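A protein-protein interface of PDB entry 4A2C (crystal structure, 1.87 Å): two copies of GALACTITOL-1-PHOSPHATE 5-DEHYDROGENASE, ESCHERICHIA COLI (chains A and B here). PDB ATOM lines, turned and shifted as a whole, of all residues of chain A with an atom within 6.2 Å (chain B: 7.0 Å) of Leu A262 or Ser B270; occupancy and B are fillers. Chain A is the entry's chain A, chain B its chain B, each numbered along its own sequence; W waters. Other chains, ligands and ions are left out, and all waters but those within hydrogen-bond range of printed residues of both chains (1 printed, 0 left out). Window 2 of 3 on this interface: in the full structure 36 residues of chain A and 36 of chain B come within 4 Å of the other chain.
No position is printed for both chains.
Hydrophobic or aromatic side chains of chain B within 4 Å of the printed part of chain A: His B267, Leu B268, Phe B273 and Leu B277. Of the 12 printed residues of chain A, 7 touch a printed residue of chain B. Hydrophobic or aromatic side chains of chain A within 4 Å of the printed part of chain B: Val A243, Leu A262 and Leu A266. Among the printed residues, 13 pairs touch across the chains. Among the printed residues, no Asp or Glu carboxylate lies within 4 Å of a Lys or Arg side-chain nitrogen of the other chain.
OD2 of Asp A265 is in hydrogen-bond range of NE2 of His B267, at 2.7 Å. OD1 of Asp A265 lies within hydrogen-bond range of N of Ser B270, at 3.2 Å. O of Leu A266 sits at hydrogen-bond distance from N of Leu B268 (2.6 Å).
CZ of Phe B273 touches CG2 of Val A243, at 3.9 Å. Gly A260 touches Phe B273. CD2 of Leu B277 touches O of Gly A260, at 3.5 Å. Leu B277 touches Thr A261. Leu A262 touches Ser B270. Phe B273 touches Leu A262. O of Gln A264 touches CB of Ser B270, at 3.7 Å. Asp A265 touches Leu B268. Asp A265 touches Thr B269. Leu A266 touches His B267 (O to CA, 3.4 Å).
O of Glu A235 lies within hydrogen-bond range of N of Gly A260 (3.1 Å). The side-chain hydroxyl (OG1) of Thr B272 is in hydrogen-bond range of the backbone carbonyl oxygen (O) of Thr B269 (2.6 Å).
Water W1 bridges O of Leu A262 (2.8 Å) and O of Ser B270 (2.8 Å).
Glu A235 touches none of the printed residues of chain B. Of the printed residues of chain B, Gly A260 touches Phe B273 and Leu B277. Leu A262 touches just these residues of chain B: Ser B270 and Phe B273. Printed residues of chain B within 4 Å of Leu A266: His B267 and Leu B268. Of chain A, only Leu A262, Gln A264 and Asp A265 come within 4 Å of Ser B270. Of the printed residues of chain A, Phe B273 touches Val A243 (3.9 Å), Gly A260 (3.5 Å) and Leu A262 (3.4 Å). Lys B275 touches none of the printed residues of chain A. Of the printed residues of chain A, Leu B277 touches Gly A260 and Thr A261. The nearest printed residue of chain B that does not touch Leu A262 is Thr B269 (5.7 Å).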
ATOM      1  N   GLU A 235       4.460 -12.577 -15.780  1.00  0.00           N
ATOM      2  CA  GLU A 235       3.352 -12.760 -16.701  1.00  0.00           C
ATOM      3  C   GLU A 235       2.273 -11.720 -16.390  1.00  0.00           C
ATOM      4  O   GLU A 235       1.574 -11.810 -15.371  1.00  0.00           O
ATOM      5  CB  GLU A 235       2.797 -14.188 -16.571  1.00  0.00           C
ATOM      6  CG  GLU A 235       1.988 -14.639 -17.794  1.00  0.00           C
ATOM      7  CD  GLU A 235       0.926 -13.623 -18.180  1.00  0.00           C
ATOM      8  OE1 GLU A 235      -0.048 -13.450 -17.407  1.00  0.00           O
ATOM      9  OE2 GLU A 235       1.058 -12.977 -19.252  1.00  0.00           O
ATOM     10  N   GLY A 238      -2.145 -12.044 -18.678  1.00  0.00           N
ATOM     11  CA  GLY A 238      -3.325 -12.752 -18.217  1.00  0.00           C
ATOM     12  C   GLY A 238      -4.122 -13.440 -19.319  1.00  0.00           C
ATOM     13  O   GLY A 238      -5.345 -13.270 -19.404  1.00  0.00           O
ATOM     14  N   VAL A 239      -3.432 -14.198 -20.171  1.00  0.00           N
ATOM     15  CA  VAL A 239      -4.098 -15.067 -21.142  1.00  0.00           C
ATOM     16  C   VAL A 239      -3.410 -16.440 -21.172  1.00  0.00           C
ATOM     17  O   VAL A 239      -2.188 -16.531 -21.004  1.00  0.00           O
ATOM     18  CB  VAL A 239      -4.130 -14.451 -22.569  1.00  0.00           C
ATOM     19  CG1 VAL A 239      -4.827 -13.089 -22.562  1.00  0.00           C
ATOM     20  CG2 VAL A 239      -2.718 -14.341 -23.133  1.00  0.00           C
ATOM     21  N   PRO A 240      -4.190 -17.510 -21.374  1.00  0.00           N
ATOM     22  CA  PRO A 240      -3.632 -18.873 -21.371  1.00  0.00           C
ATOM     23  C   PRO A 240      -2.345 -18.979 -22.193  1.00  0.00           C
ATOM     24  O   PRO A 240      -1.388 -19.618 -21.754  1.00  0.00           O
ATOM     25  CB  PRO A 240      -4.743 -19.699 -22.022  1.00  0.00           C
ATOM     26  CG  PRO A 240      -6.004 -18.980 -21.631  1.00  0.00           C
ATOM     27  CD  PRO A 240      -5.644 -17.509 -21.627  1.00  0.00           C
ATOM     28  N   VAL A 243       0.733 -17.546 -20.306  1.00  0.00           N
ATOM     29  CA  VAL A 243       1.122 -18.423 -19.189  1.00  0.00           C
ATOM     30  C   VAL A 243       1.869 -19.650 -19.737  1.00  0.00           C
ATOM     31  O   VAL A 243       2.926 -20.035 -19.235  1.00  0.00           O
ATOM     32  CB  VAL A 243      -0.096 -18.874 -18.353  1.00  0.00           C
ATOM     33  CG1 VAL A 243       0.303 -19.999 -17.370  1.00  0.00           C
ATOM     34  CG2 VAL A 243      -0.720 -17.673 -17.622  1.00  0.00           C
ATOM     35  N   GLY A 260      -1.110 -11.643 -13.919  1.00  0.00           N
ATOM     36  CA  GLY A 260      -2.245 -11.567 -14.815  1.00  0.00           C
ATOM     37  C   GLY A 260      -3.319 -12.610 -14.571  1.00  0.00           C
ATOM     38  O   GLY A 260      -3.091 -13.812 -14.681  1.00  0.00           O
ATOM     39  N   THR A 261      -4.516 -12.133 -14.257  1.00  0.00           N
ATOM     40  CA  THR A 261      -5.674 -12.993 -14.072  1.00  0.00           C
ATOM     41  C   THR A 261      -6.215 -13.512 -15.405  1.00  0.00           C
ATOM     42  O   THR A 261      -6.359 -12.754 -16.365  1.00  0.00           O
ATOM     43  CB  THR A 261      -6.788 -12.230 -13.341  1.00  0.00           C
ATOM     44  OG1 THR A 261      -6.352 -11.935 -12.007  1.00  0.00           O
ATOM     45  CG2 THR A 261      -8.052 -13.063 -13.286  1.00  0.00           C
ATOM     46  N   LEU A 262      -6.504 -14.810 -15.458  1.00  0.00           N
ATOM     47  CA  LEU A 262      -7.110 -15.432 -16.636  1.00  0.00           C
ATOM     48  C   LEU A 262      -8.629 -15.250 -16.651  1.00  0.00           C
ATOM     49  O   LEU A 262      -9.261 -15.156 -15.595  1.00  0.00           O
ATOM     50  CB  LEU A 262      -6.787 -16.931 -16.677  1.00  0.00           C
ATOM     51  CG  LEU A 262      -5.543 -17.367 -17.442  1.00  0.00           C
ATOM     52  CD1 LEU A 262      -4.361 -16.468 -17.136  1.00  0.00           C
ATOM     53  CD2 LEU A 262      -5.209 -18.828 -17.144  1.00  0.00           C
ATOM     54  N   HIS A 263      -9.210 -15.177 -17.848  1.00  0.00           N
ATOM     55  CA  HIS A 263     -10.660 -15.256 -17.980  1.00  0.00           C
ATOM     56  C   HIS A 263     -11.062 -16.392 -18.917  1.00  0.00           C
ATOM     57  O   HIS A 263     -12.250 -16.617 -19.162  1.00  0.00           O
ATOM     58  CB  HIS A 263     -11.258 -13.914 -18.417  1.00  0.00           C
ATOM     59  CG  HIS A 263     -11.097 -12.835 -17.393  1.00  0.00           C
ATOM     60  ND1 HIS A 263     -10.034 -11.956 -17.395  1.00  0.00           N
ATOM     61  CD2 HIS A 263     -11.847 -12.516 -16.309  1.00  0.00           C
ATOM     62  CE1 HIS A 263     -10.147 -11.131 -16.369  1.00  0.00           C
ATOM     63  NE2 HIS A 263     -11.239 -11.448 -15.695  1.00  0.00           N
ATOM     64  N   GLN A 264     -10.060 -17.094 -19.443  1.00  0.00           N
ATOM     65  CA  GLN A 264     -10.276 -18.335 -20.165  1.00  0.00           C
ATOM     66  C   GLN A 264      -9.525 -19.425 -19.427  1.00  0.00           C
ATOM     67  O   GLN A 264      -8.568 -19.138 -18.699  1.00  0.00           O
ATOM     68  CB  GLN A 264      -9.745 -18.236 -21.590  1.00  0.00           C
ATOM     69  CG  GLN A 264     -10.821 -18.209 -22.644  1.00  0.00           C
ATOM     70  CD  GLN A 264     -10.432 -17.361 -23.837  1.00  0.00           C
ATOM     71  OE1 GLN A 264      -9.613 -16.446 -23.719  1.00  0.00           O
ATOM     72  NE2 GLN A 264     -11.015 -17.661 -24.996  1.00  0.00           N
ATOM     73  N   ASP A 265      -9.941 -20.672 -19.616  1.00  0.00           N
ATOM     74  CA  ASP A 265      -9.277 -21.790 -18.953  1.00  0.00           C
ATOM     75  C   ASP A 265      -7.850 -21.959 -19.440  1.00  0.00           C
ATOM     76  O   ASP A 265      -7.514 -21.595 -20.573  1.00  0.00           O
ATOM     77  CB  ASP A 265     -10.018 -23.097 -19.211  1.00  0.00           C
ATOM     78  CG  ASP A 265     -11.363 -23.150 -18.530  1.00  0.00           C
ATOM     79  OD1 ASP A 265     -11.672 -22.236 -17.731  1.00  0.00           O
ATOM     80  OD2 ASP A 265     -12.099 -24.118 -18.800  1.00  0.00           O
ATOM     81  N   LEU A 266      -7.018 -22.536 -18.582  1.00  0.00           N
ATOM     82  CA  LEU A 266      -5.654 -22.865 -18.958  1.00  0.00           C
ATOM     83  C   LEU A 266      -5.558 -24.343 -19.348  1.00  0.00           C
ATOM     84  O   LEU A 266      -5.958 -25.224 -18.590  1.00  0.00           O
ATOM     85  CB  LEU A 266      -4.704 -22.568 -17.795  1.00  0.00           C
ATOM     86  CG  LEU A 266      -3.225 -22.787 -18.109  1.00  0.00           C
ATOM     87  CD1 LEU A 266      -2.809 -21.873 -19.227  1.00  0.00           C
ATOM     88  CD2 LEU A 266      -2.352 -22.563 -16.874  1.00  0.00           C
ATOM     89  N   HIS B 267      -6.103 -29.493 -17.743  1.00  0.00           N
ATOM     90  CA  HIS B 267      -7.004 -28.399 -18.074  1.00  0.00           C
ATOM     91  C   HIS B 267      -7.442 -27.734 -16.769  1.00  0.00           C
ATOM     92  O   HIS B 267      -8.145 -28.341 -15.966  1.00  0.00           O
ATOM     93  CB  HIS B 267      -8.209 -28.913 -18.863  1.00  0.00           C
ATOM     94  CG  HIS B 267      -9.160 -27.836 -19.275  1.00  0.00           C
ATOM     95  ND1 HIS B 267      -9.041 -27.148 -20.462  1.00  0.00           N
ATOM     96  CD2 HIS B 267     -10.247 -27.320 -18.650  1.00  0.00           C
ATOM     97  CE1 HIS B 267     -10.019 -26.263 -20.560  1.00  0.00           C
ATOM     98  NE2 HIS B 267     -10.760 -26.345 -19.468  1.00  0.00           N
ATOM     99  N   LEU B 268      -6.997 -26.498 -16.549  1.00  0.00           N
ATOM    100  CA  LEU B 268      -7.311 -25.761 -15.327  1.00  0.00           C
ATOM    101  C   LEU B 268      -8.333 -24.670 -15.635  1.00  0.00           C
ATOM    102  O   LEU B 268      -8.150 -23.885 -16.573  1.00  0.00           O
ATOM    103  CB  LEU B 268      -6.052 -25.099 -14.746  1.00  0.00           C
ATOM    104  CG  LEU B 268      -5.229 -25.779 -13.651  1.00  0.00           C
ATOM    105  CD1 LEU B 268      -4.137 -24.836 -13.169  1.00  0.00           C
ATOM    106  CD2 LEU B 268      -6.103 -26.216 -12.479  1.00  0.00           C
ATOM    107  N   THR B 269      -9.407 -24.620 -14.854  1.00  0.00           N
ATOM    108  CA  THR B 269     -10.381 -23.543 -14.991  1.00  0.00           C
ATOM    109  C   THR B 269      -9.692 -22.231 -14.680  1.00  0.00           C
ATOM    110  O   THR B 269      -8.621 -22.219 -14.064  1.00  0.00           O
ATOM    111  CB  THR B 269     -11.576 -23.710 -14.030  1.00  0.00           C
ATOM    112  OG1 THR B 269     -11.126 -23.553 -12.678  1.00  0.00           O
ATOM    113  CG2 THR B 269     -12.221 -25.079 -14.216  1.00  0.00           C
ATOM    114  N   SER B 270     -10.288 -21.127 -15.117  1.00  0.00           N
ATOM    115  CA  SER B 270      -9.731 -19.811 -14.806  1.00  0.00           C
ATOM    116  C   SER B 270      -9.829 -19.568 -13.306  1.00  0.00           C
ATOM    117  O   SER B 270      -8.910 -19.023 -12.696  1.00  0.00           O
ATOM    118  CB  SER B 270     -10.474 -18.706 -15.556  1.00  0.00           C
ATOM    119  OG  SER B 270     -11.723 -18.431 -14.936  1.00  0.00           O
ATOM    120  N   ALA B 271     -10.939 -19.991 -12.706  1.00  0.00           N
ATOM    121  CA  ALA B 271     -11.116 -19.838 -11.258  1.00  0.00           C
ATOM    122  C   ALA B 271      -9.986 -20.535 -10.497  1.00  0.00           C
ATOM    123  O   ALA B 271      -9.346 -19.947  -9.625  1.00  0.00           O
ATOM    124  CB  ALA B 271     -12.461 -20.390 -10.827  1.00  0.00           C
ATOM    125  N   THR B 272      -9.739 -21.795 -10.829  1.00  0.00           N
ATOM    126  CA  THR B 272      -8.665 -22.535 -10.171  1.00  0.00           C
ATOM    127  C   THR B 272      -7.323 -21.820 -10.335  1.00  0.00           C
ATOM    128  O   THR B 272      -6.611 -21.561  -9.354  1.00  0.00           O
ATOM    129  CB  THR B 272      -8.557 -23.974 -10.714  1.00  0.00           C
ATOM    130  OG1 THR B 272      -8.526 -23.940 -12.149  1.00  0.00           O
ATOM    131  CG2 THR B 272      -9.747 -24.788 -10.275  1.00  0.00           C
ATOM    132  N   PHE B 273      -6.969 -21.521 -11.579  1.00  0.00           N
ATOM    133  CA  PHE B 273      -5.764 -20.742 -11.841  1.00  0.00           C
ATOM    134  C   PHE B 273      -5.809 -19.464 -11.010  1.00  0.00           C
ATOM    135  O   PHE B 273      -4.798 -19.060 -10.426  1.00  0.00           O
ATOM    136  CB  PHE B 273      -5.643 -20.393 -13.327  1.00  0.00           C
ATOM    137  CG  PHE B 273      -4.532 -19.419 -13.631  1.00  0.00           C
ATOM    138  CD1 PHE B 273      -4.750 -18.050 -13.554  1.00  0.00           C
ATOM    139  CD2 PHE B 273      -3.275 -19.872 -13.991  1.00  0.00           C
ATOM    140  CE1 PHE B 273      -3.737 -17.153 -13.829  1.00  0.00           C
ATOM    141  CE2 PHE B 273      -2.247 -18.977 -14.274  1.00  0.00           C
ATOM    142  CZ  PHE B 273      -2.481 -17.612 -14.194  1.00  0.00           C
ATOM    143  N   GLY B 274      -6.987 -18.846 -10.945  1.00  0.00           N
ATOM    144  CA  GLY B 274      -7.156 -17.612 -10.199  1.00  0.00           C
ATOM    145  C   GLY B 274      -6.678 -17.729  -8.761  1.00  0.00           C
ATOM    146  O   GLY B 274      -6.104 -16.779  -8.217  1.00  0.00           O
ATOM    147  N   LYS B 275      -6.915 -18.890  -8.146  1.00  0.00           N
ATOM    148  CA  LYS B 275      -6.537 -19.118  -6.746  1.00  0.00           C
ATOM    149  C   LYS B 275      -5.025 -19.149  -6.532  1.00  0.00           C
ATOM    150  O   LYS B 275      -4.543 -18.860  -5.427  1.00  0.00           O
ATOM    151  CB  LYS B 275      -7.213 -20.384  -6.170  1.00  0.00           C
ATOM    152  CG  LYS B 275      -8.748 -20.323  -6.158  1.00  0.00           C
ATOM    153  CD  LYS B 275      -9.383 -21.515  -5.427  1.00  0.00           C
ATOM    154  CE  LYS B 275     -10.880 -21.279  -5.224  1.00  0.00           C
ATOM    155  NZ  LYS B 275     -11.520 -22.253  -4.280  1.00  0.00           N
ATOM    156  N   ILE B 276      -4.251 -19.500  -7.560  1.00  0.00           N
ATOM    157  CA  ILE B 276      -2.808 -19.471  -7.356  1.00  0.00           C
ATOM    158  C   ILE B 276      -2.400 -18.010  -7.093  1.00  0.00           C
ATOM    159  O   ILE B 276      -1.619 -17.713  -6.189  1.00  0.00           O
ATOM    160  CB  ILE B 276      -2.025 -20.061  -8.533  1.00  0.00           C
ATOM    161  CG1 ILE B 276      -2.469 -21.512  -8.779  1.00  0.00           C
ATOM    162  CG2 ILE B 276      -0.510 -20.002  -8.229  1.00  0.00           C
ATOM    163  CD1 ILE B 276      -2.194 -22.025 -10.184  1.00  0.00           C
ATOM    164  N   LEU B 277      -2.962 -17.093  -7.866  1.00  0.00           N
ATOM    165  CA  LEU B 277      -2.667 -15.683  -7.645  1.00  0.00           C
ATOM    166  C   LEU B 277      -3.252 -15.233  -6.294  1.00  0.00           C
ATOM    167  O   LEU B 277      -2.540 -14.664  -5.454  1.00  0.00           O
ATOM    168  CB  LEU B 277      -3.188 -14.824  -8.814  1.00  0.00           C
ATOM    169  CG  LEU B 277      -2.357 -14.829 -10.113  1.00  0.00           C
ATOM    170  CD1 LEU B 277      -2.280 -16.217 -10.754  1.00  0.00           C
ATOM    171  CD2 LEU B 277      -2.881 -13.812 -11.150  1.00  0.00           C
HETATM  172  O   HOH W   1      -8.143 -16.378 -13.322  1.00  0.00           O
